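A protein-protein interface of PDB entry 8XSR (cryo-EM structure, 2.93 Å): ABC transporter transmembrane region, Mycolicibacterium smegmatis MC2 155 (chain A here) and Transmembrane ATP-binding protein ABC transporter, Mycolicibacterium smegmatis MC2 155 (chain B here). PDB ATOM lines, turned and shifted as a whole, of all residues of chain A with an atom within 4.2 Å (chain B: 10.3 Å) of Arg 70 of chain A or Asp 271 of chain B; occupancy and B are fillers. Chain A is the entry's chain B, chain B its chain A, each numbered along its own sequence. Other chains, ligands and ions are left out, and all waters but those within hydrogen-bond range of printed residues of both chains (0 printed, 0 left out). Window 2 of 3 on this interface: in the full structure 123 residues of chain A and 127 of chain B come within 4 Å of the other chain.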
ATOM      1  N   GLY A  66      27.617  33.413   9.105  1.00  0.00           N
ATOM      2  CA  GLY A  66      28.909  32.792   8.927  1.00  0.00           C
ATOM      3  C   GLY A  66      28.809  31.333   8.553  1.00  0.00           C
ATOM      4  O   GLY A  66      29.735  30.775   7.962  1.00  0.00           O
ATOM      5  N   VAL A  67      27.693  30.698   8.893  1.00  0.00           N
ATOM      6  CA  VAL A  67      27.515  29.299   8.532  1.00  0.00           C
ATOM      7  C   VAL A  67      27.110  29.125   7.074  1.00  0.00           C
ATOM      8  O   VAL A  67      27.665  28.265   6.382  1.00  0.00           O
ATOM      9  CB  VAL A  67      26.506  28.631   9.473  1.00  0.00           C
ATOM     10  CG1 VAL A  67      26.132  27.262   8.956  1.00  0.00           C
ATOM     11  CG2 VAL A  67      27.128  28.499  10.828  1.00  0.00           C
ATOM     12  N   ILE A  68      26.173  29.925   6.570  1.00  0.00           N
ATOM     13  CA  ILE A  68      25.833  29.793   5.157  1.00  0.00           C
ATOM     14  C   ILE A  68      26.542  30.890   4.379  1.00  0.00           C
ATOM     15  O   ILE A  68      26.111  31.277   3.288  1.00  0.00           O
ATOM     16  CB  ILE A  68      24.315  29.817   4.907  1.00  0.00           C
ATOM     17  CG1 ILE A  68      23.709  31.156   5.286  1.00  0.00           C
ATOM     18  CG2 ILE A  68      23.625  28.698   5.668  1.00  0.00           C
ATOM     19  CD1 ILE A  68      22.315  31.286   4.773  1.00  0.00           C
ATOM     20  N   GLY A  69      27.639  31.392   4.936  1.00  0.00           N
ATOM     21  CA  GLY A  69      28.460  32.366   4.250  1.00  0.00           C
ATOM     22  C   GLY A  69      29.906  31.933   4.155  1.00  0.00           C
ATOM     23  O   GLY A  69      30.736  32.643   3.582  1.00  0.00           O
ATOM     24  N   ARG A  70      30.222  30.765   4.712  1.00  0.00           N
ATOM     25  CA  ARG A  70      31.557  30.202   4.585  1.00  0.00           C
ATOM     26  C   ARG A  70      31.616  29.067   3.577  1.00  0.00           C
ATOM     27  O   ARG A  70      32.719  28.650   3.209  1.00  0.00           O
ATOM     28  CB  ARG A  70      32.066  29.694   5.941  1.00  0.00           C
ATOM     29  CG  ARG A  70      31.309  28.486   6.454  1.00  0.00           C
ATOM     30  CD  ARG A  70      31.797  28.055   7.824  1.00  0.00           C
ATOM     31  NE  ARG A  70      31.056  26.896   8.310  1.00  0.00           N
ATOM     32  CZ  ARG A  70      31.277  26.302   9.476  1.00  0.00           C
ATOM     33  NH1 ARG A  70      32.224  26.757  10.282  1.00  0.00           N
ATOM     34  NH2 ARG A  70      30.552  25.252   9.835  1.00  0.00           N
ATOM     35  N   GLU A  71      30.475  28.548   3.128  1.00  0.00           N
ATOM     36  CA  GLU A  71      30.427  27.547   2.077  1.00  0.00           C
ATOM     37  C   GLU A  71      30.508  28.168   0.690  1.00  0.00           C
ATOM     38  O   GLU A  71      30.803  27.458  -0.279  1.00  0.00           O
ATOM     39  CB  GLU A  71      29.142  26.717   2.212  1.00  0.00           C
ATOM     40  CG  GLU A  71      29.031  25.529   1.269  1.00  0.00           C
ATOM     41  CD  GLU A  71      30.068  24.461   1.552  1.00  0.00           C
ATOM     42  OE1 GLU A  71      30.524  24.365   2.710  1.00  0.00           O
ATOM     43  OE2 GLU A  71      30.430  23.719   0.614  1.00  0.00           O
ATOM     44  N   LEU A  72      30.288  29.470   0.578  1.00  0.00           N
ATOM     45  CA  LEU A  72      30.402  30.210  -0.664  1.00  0.00           C
ATOM     46  C   LEU A  72      31.864  30.380  -1.047  1.00  0.00           C
ATOM     47  O   LEU A  72      32.748  30.372  -0.185  1.00  0.00           O
ATOM     48  CB  LEU A  72      29.737  31.575  -0.520  1.00  0.00           C
ATOM     49  CG  LEU A  72      28.226  31.571  -0.298  1.00  0.00           C
ATOM     50  CD1 LEU A  72      27.741  32.974  -0.024  1.00  0.00           C
ATOM     51  CD2 LEU A  72      27.508  30.984  -1.497  1.00  0.00           C
ATOM     52  N   GLN A 106      34.254  34.028   5.009  1.00  0.00           N
ATOM     53  CA  GLN A 106      34.512  34.229   6.426  1.00  0.00           C
ATOM     54  C   GLN A 106      33.668  33.292   7.283  1.00  0.00           C
ATOM     55  O   GLN A 106      32.609  32.812   6.873  1.00  0.00           O
ATOM     56  CB  GLN A 106      34.249  35.677   6.834  1.00  0.00           C
ATOM     57  CG  GLN A 106      35.242  36.669   6.269  1.00  0.00           C
ATOM     58  CD  GLN A 106      35.005  38.075   6.778  1.00  0.00           C
ATOM     59  OE1 GLN A 106      34.055  38.326   7.518  1.00  0.00           O
ATOM     60  NE2 GLN A 106      35.874  39.000   6.391  1.00  0.00           N
ATOM     61  N   VAL A 108      32.514  32.607  11.619  1.00  0.00           N
ATOM     62  CA  VAL A 108      31.492  33.080  12.545  1.00  0.00           C
ATOM     63  C   VAL A 108      31.901  34.399  13.191  1.00  0.00           C
ATOM     64  O   VAL A 108      31.045  35.239  13.496  1.00  0.00           O
ATOM     65  CB  VAL A 108      31.191  32.010  13.610  1.00  0.00           C
ATOM     66  CG1 VAL A 108      30.245  32.547  14.654  1.00  0.00           C
ATOM     67  CG2 VAL A 108      30.597  30.776  12.956  1.00  0.00           C
ATOM     68  N   PHE A 110      33.596  34.859  16.301  1.00  0.00           N
ATOM     69  CA  PHE A 110      33.126  34.754  17.679  1.00  0.00           C
ATOM     70  C   PHE A 110      33.473  35.960  18.539  1.00  0.00           C
ATOM     71  O   PHE A 110      33.020  36.019  19.683  1.00  0.00           O
ATOM     72  CB  PHE A 110      33.679  33.495  18.340  1.00  0.00           C
ATOM     73  CG  PHE A 110      33.038  32.238  17.859  1.00  0.00           C
ATOM     74  CD1 PHE A 110      31.798  31.860  18.336  1.00  0.00           C
ATOM     75  CD2 PHE A 110      33.670  31.435  16.934  1.00  0.00           C
ATOM     76  CE1 PHE A 110      31.199  30.704  17.896  1.00  0.00           C
ATOM     77  CE2 PHE A 110      33.076  30.278  16.494  1.00  0.00           C
ATOM     78  CZ  PHE A 110      31.839  29.911  16.973  1.00  0.00           C
ATOM     79  N   ASP B 160      19.633  17.310  18.967  1.00  0.00           N
ATOM     80  CA  ASP B 160      20.946  17.776  19.402  1.00  0.00           C
ATOM     81  C   ASP B 160      21.285  17.280  20.801  1.00  0.00           C
ATOM     82  O   ASP B 160      21.381  18.075  21.740  1.00  0.00           O
ATOM     83  CB  ASP B 160      21.026  19.300  19.359  1.00  0.00           C
ATOM     84  CG  ASP B 160      22.442  19.809  19.514  1.00  0.00           C
ATOM     85  OD1 ASP B 160      23.374  18.981  19.600  1.00  0.00           O
ATOM     86  OD2 ASP B 160      22.623  21.040  19.567  1.00  0.00           O
ATOM     87  N   LEU B 262      23.137  29.154  25.990  1.00  0.00           N
ATOM     88  CA  LEU B 262      22.693  28.347  24.864  1.00  0.00           C
ATOM     89  C   LEU B 262      23.364  28.778  23.575  1.00  0.00           C
ATOM     90  O   LEU B 262      23.940  27.956  22.863  1.00  0.00           O
ATOM     91  CB  LEU B 262      21.179  28.454  24.727  1.00  0.00           C
ATOM     92  CG  LEU B 262      20.600  27.698  23.542  1.00  0.00           C
ATOM     93  CD1 LEU B 262      20.799  26.222  23.745  1.00  0.00           C
ATOM     94  CD2 LEU B 262      19.148  28.041  23.379  1.00  0.00           C
ATOM     95  N   ILE B 263      23.302  30.071  23.255  1.00  0.00           N
ATOM     96  CA  ILE B 263      23.817  30.501  21.964  1.00  0.00           C
ATOM     97  C   ILE B 263      25.332  30.410  21.918  1.00  0.00           C
ATOM     98  O   ILE B 263      25.893  30.062  20.882  1.00  0.00           O
ATOM     99  CB  ILE B 263      23.308  31.907  21.620  1.00  0.00           C
ATOM    100  CG1 ILE B 263      21.810  31.838  21.370  1.00  0.00           C
ATOM    101  CG2 ILE B 263      24.006  32.453  20.393  1.00  0.00           C
ATOM    102  CD1 ILE B 263      21.198  33.151  21.129  1.00  0.00           C
ATOM    103  N   TRP B 264      26.021  30.644  23.033  1.00  0.00           N
ATOM    104  CA  TRP B 264      27.470  30.469  23.027  1.00  0.00           C
ATOM    105  C   TRP B 264      27.848  29.008  22.806  1.00  0.00           C
ATOM    106  O   TRP B 264      28.536  28.668  21.830  1.00  0.00           O
ATOM    107  CB  TRP B 264      28.074  30.995  24.328  1.00  0.00           C
ATOM    108  CG  TRP B 264      29.567  30.887  24.366  1.00  0.00           C
ATOM    109  CD1 TRP B 264      30.307  30.013  25.104  1.00  0.00           C
ATOM    110  CD2 TRP B 264      30.500  31.660  23.606  1.00  0.00           C
ATOM    111  NE1 TRP B 264      31.643  30.207  24.866  1.00  0.00           N
ATOM    112  CE2 TRP B 264      31.788  31.211  23.946  1.00  0.00           C
ATOM    113  CE3 TRP B 264      30.370  32.691  22.674  1.00  0.00           C
ATOM    114  CZ2 TRP B 264      32.937  31.758  23.390  1.00  0.00           C
ATOM    115  CZ3 TRP B 264      31.511  33.232  22.123  1.00  0.00           C
ATOM    116  CH2 TRP B 264      32.777  32.765  22.482  1.00  0.00           C
ATOM    117  N   PHE B 265      27.407  28.122  23.703  1.00  0.00           N
ATOM    118  CA  PHE B 265      27.796  26.723  23.599  1.00  0.00           C
ATOM    119  C   PHE B 265      27.139  26.014  22.426  1.00  0.00           C
ATOM    120  O   PHE B 265      27.506  24.870  22.139  1.00  0.00           O
ATOM    121  CB  PHE B 265      27.474  25.984  24.895  1.00  0.00           C
ATOM    122  CG  PHE B 265      28.291  26.435  26.065  1.00  0.00           C
ATOM    123  CD1 PHE B 265      29.603  26.026  26.208  1.00  0.00           C
ATOM    124  CD2 PHE B 265      27.747  27.260  27.027  1.00  0.00           C
ATOM    125  CE1 PHE B 265      30.355  26.440  27.282  1.00  0.00           C
ATOM    126  CE2 PHE B 265      28.494  27.675  28.103  1.00  0.00           C
ATOM    127  CZ  PHE B 265      29.798  27.266  28.231  1.00  0.00           C
ATOM    128  N   GLY B 266      26.194  26.652  21.743  1.00  0.00           N
ATOM    129  CA  GLY B 266      25.584  26.069  20.573  1.00  0.00           C
ATOM    130  C   GLY B 266      26.198  26.598  19.301  1.00  0.00           C
ATOM    131  O   GLY B 266      26.288  25.870  18.317  1.00  0.00           O
ATOM    132  N   GLY B 267      26.634  27.857  19.297  1.00  0.00           N
ATOM    133  CA  GLY B 267      27.399  28.356  18.175  1.00  0.00           C
ATOM    134  C   GLY B 267      28.768  27.727  18.094  1.00  0.00           C
ATOM    135  O   GLY B 267      29.316  27.570  17.001  1.00  0.00           O
ATOM    136  N   LEU B 268      29.337  27.350  19.242  1.00  0.00           N
ATOM    137  CA  LEU B 268      30.575  26.581  19.204  1.00  0.00           C
ATOM    138  C   LEU B 268      30.397  25.248  18.488  1.00  0.00           C
ATOM    139  O   LEU B 268      31.361  24.732  17.915  1.00  0.00           O
ATOM    140  CB  LEU B 268      31.108  26.350  20.616  1.00  0.00           C
ATOM    141  CG  LEU B 268      31.589  27.600  21.347  1.00  0.00           C
ATOM    142  CD1 LEU B 268      32.030  27.254  22.757  1.00  0.00           C
ATOM    143  CD2 LEU B 268      32.712  28.263  20.574  1.00  0.00           C
ATOM    144  N   ARG B 269      29.191  24.681  18.508  1.00  0.00           N
ATOM    145  CA  ARG B 269      28.898  23.462  17.766  1.00  0.00           C
ATOM    146  C   ARG B 269      28.453  23.736  16.339  1.00  0.00           C
ATOM    147  O   ARG B 269      28.734  22.933  15.444  1.00  0.00           O
ATOM    148  CB  ARG B 269      27.808  22.659  18.478  1.00  0.00           C
ATOM    149  CG  ARG B 269      28.223  22.084  19.811  1.00  0.00           C
ATOM    150  CD  ARG B 269      27.057  21.387  20.477  1.00  0.00           C
ATOM    151  NE  ARG B 269      26.593  20.245  19.699  1.00  0.00           N
ATOM    152  CZ  ARG B 269      27.087  19.019  19.811  1.00  0.00           C
ATOM    153  NH1 ARG B 269      28.065  18.776  20.671  1.00  0.00           N
ATOM    154  NH2 ARG B 269      26.607  18.037  19.065  1.00  0.00           N
ATOM    155  N   ILE B 270      27.755  24.848  16.113  1.00  0.00           N
ATOM    156  CA  ILE B 270      27.289  25.184  14.774  1.00  0.00           C
ATOM    157  C   ILE B 270      28.466  25.536  13.873  1.00  0.00           C
ATOM    158  O   ILE B 270      28.486  25.179  12.691  1.00  0.00           O
ATOM    159  CB  ILE B 270      26.251  26.319  14.838  1.00  0.00           C
ATOM    160  CG1 ILE B 270      24.988  25.851  15.555  1.00  0.00           C
ATOM    161  CG2 ILE B 270      25.863  26.757  13.467  1.00  0.00           C
ATOM    162  CD1 ILE B 270      24.024  26.969  15.866  1.00  0.00           C
ATOM    163  N   ASP B 271      29.468  26.232  14.416  1.00  0.00           N
ATOM    164  CA  ASP B 271      30.694  26.451  13.658  1.00  0.00           C
ATOM    165  C   ASP B 271      31.408  25.132  13.385  1.00  0.00           C
ATOM    166  O   ASP B 271      31.898  24.900  12.275  1.00  0.00           O
ATOM    167  CB  ASP B 271      31.618  27.408  14.409  1.00  0.00           C
ATOM    168  CG  ASP B 271      32.794  27.869  13.563  1.00  0.00           C
ATOM    169  OD1 ASP B 271      32.879  27.477  12.382  1.00  0.00           O
ATOM    170  OD2 ASP B 271      33.647  28.615  14.081  1.00  0.00           O
ATOM    171  N   ALA B 272      31.468  24.252  14.384  1.00  0.00           N
ATOM    172  CA  ALA B 272      32.135  22.967  14.227  1.00  0.00           C
ATOM    173  C   ALA B 272      31.394  22.020  13.292  1.00  0.00           C
ATOM    174  O   ALA B 272      31.851  20.889  13.099  1.00  0.00           O
ATOM    175  CB  ALA B 272      32.321  22.305  15.591  1.00  0.00           C
ATOM    176  N   GLY B 273      30.271  22.441  12.716  1.00  0.00           N
ATOM    177  CA  GLY B 273      29.546  21.615  11.776  1.00  0.00           C
ATOM    178  C   GLY B 273      28.749  20.488  12.388  1.00  0.00           C
ATOM    179  O   GLY B 273      28.213  19.658  11.646  1.00  0.00           O
ATOM    180  N   GLN B 274      28.643  20.435  13.712  1.00  0.00           N
ATOM    181  CA  GLN B 274      27.967  19.349  14.404  1.00  0.00           C
ATOM    182  C   GLN B 274      26.650  19.778  15.036  1.00  0.00           C
ATOM    183  O   GLN B 274      26.174  19.118  15.964  1.00  0.00           O
ATOM    184  CB  GLN B 274      28.900  18.752  15.457  1.00  0.00           C
ATOM    185  CG  GLN B 274      29.356  19.741  16.508  1.00  0.00           C
ATOM    186  CD  GLN B 274      30.392  19.158  17.443  1.00  0.00           C
ATOM    187  OE1 GLN B 274      30.745  17.984  17.343  1.00  0.00           O
ATOM    188  NE2 GLN B 274      30.892  19.978  18.357  1.00  0.00           N
ATOM    189  N   MET B 275      26.047  20.859  14.548  1.00  0.00           N
ATOM    190  CA  MET B 275      24.758  21.330  15.034  1.00  0.00           C
ATOM    191  C   MET B 275      24.135  22.203  13.958  1.00  0.00           C
ATOM    192  O   MET B 275      24.842  22.969  13.299  1.00  0.00           O
ATOM    193  CB  MET B 275      24.907  22.122  16.334  1.00  0.00           C
ATOM    194  CG  MET B 275      23.598  22.621  16.920  1.00  0.00           C
ATOM    195  SD  MET B 275      23.859  23.574  18.424  1.00  0.00           S
ATOM    196  CE  MET B 275      22.200  24.125  18.778  1.00  0.00           C
ATOM    197  N   GLN B 276      22.826  22.086  13.780  1.00  0.00           N
ATOM    198  CA  GLN B 276      22.139  22.929  12.817  1.00  0.00           C
ATOM    199  C   GLN B 276      21.668  24.218  13.484  1.00  0.00           C
ATOM    200  O   GLN B 276      21.346  24.254  14.673  1.00  0.00           O
ATOM    201  CB  GLN B 276      20.960  22.185  12.199  1.00  0.00           C
ATOM    202  CG  GLN B 276      21.363  20.947  11.417  1.00  0.00           C
ATOM    203  CD  GLN B 276      22.298  21.261  10.270  1.00  0.00           C
ATOM    204  OE1 GLN B 276      23.481  20.925  10.311  1.00  0.00           O
ATOM    205  NE2 GLN B 276      21.776  21.912   9.240  1.00  0.00           N
ATOM    206  N   VAL B 277      21.629  25.292  12.691  1.00  0.00           N
ATOM    207  CA  VAL B 277      21.275  26.605  13.218  1.00  0.00           C
ATOM    208  C   VAL B 277      19.852  26.653  13.751  1.00  0.00           C
ATOM    209  O   VAL B 277      19.556  27.464  14.634  1.00  0.00           O
ATOM    210  CB  VAL B 277      21.477  27.677  12.128  1.00  0.00           C
ATOM    211  CG1 VAL B 277      21.186  29.068  12.666  1.00  0.00           C
ATOM    212  CG2 VAL B 277      22.882  27.599  11.565  1.00  0.00           C
ATOM    213  N   LEU B 280      18.798  26.020  17.742  1.00  0.00           N
ATOM    214  CA  LEU B 280      18.715  27.087  18.729  1.00  0.00           C
ATOM    215  C   LEU B 280      17.311  27.639  18.868  1.00  0.00           C
ATOM    216  O   LEU B 280      16.873  27.925  19.989  1.00  0.00           O
ATOM    217  CB  LEU B 280      19.658  28.235  18.360  1.00  0.00           C
ATOM    218  CG  LEU B 280      21.155  27.963  18.418  1.00  0.00           C
ATOM    219  CD1 LEU B 280      21.905  29.161  17.897  1.00  0.00           C
ATOM    220  CD2 LEU B 280      21.577  27.651  19.833  1.00  0.00           C
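Of the 10 printed residues of chain A, 4 touch a printed residue of chain B. Hydrophobic or aromatic side chains of chain A within 4 Å of the printed part of chain B: Val 67, Val 108 and Phe 110. Printed residues of chain B that touch a printed residue of chain A: Trp 264, Gly 267, Leu 268, Ile 270 and Asp 271. Among the printed residues, 8 pairs touch across the chains. Among the printed residues, Asp or Glu carboxylates within 4 Å of a Lys or Arg side-chain nitrogen of the other chain: Arg 70 of chain A with Asp 271 of chain B (2.3 Å).
CG2 of Ile 270 of chain B touches CG2 of Val 67 of chain A, 3.4 Å away. Arg 70 of chain A touches Ile 270 of chain B. CG2 of Val 108 of chain A touches CG of Asp 271 of chain B, 3.7 Å away. Phe 110 of chain A touches Trp 264 of chain B. Phe 110 of chain A touches Gly 267 of chain B. Phe 110 of chain A touches Leu 268 of chain B (CE1 to CD2, 3.9 Å). Phe 110 of chain A touches Asp 271 of chain B (CE2 to OD2, 3.0 Å).
Of the printed residues of chain B, Arg 70 of chain A touches Ile 270 (3.5 Å) and Asp 271 (2.3 Å). Asp 271 of chain B touches three residues of chain A. No residue of chain B comes within 4 Å of Gly 66 of chain A. Val 67 of chain A touches just one residue of chain B: Ile 270 (3.4 Å). No residue of chain B comes within 4 Å of Gly 69 of chain A. No residue of chain B comes within 4 Å of Glu 71 of chain A. Of the printed residues of chain B, Val 108 of chain A touches Asp 271. Printed residues of chain A within 4 Å of Ile 270 of chain B: Val 67 and Arg 70. Of the printed residues of chain A, Leu 268 of chain B touches Phe 110 (3.9 Å). Met 275 of chain B touches none of the printed residues of chain A.
The guanidinium group of Arg 70 of chain A sits at hydrogen-bond distance from the backbone carbonyl oxygen of Asp 271 of chain B, at 2.7 Å.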
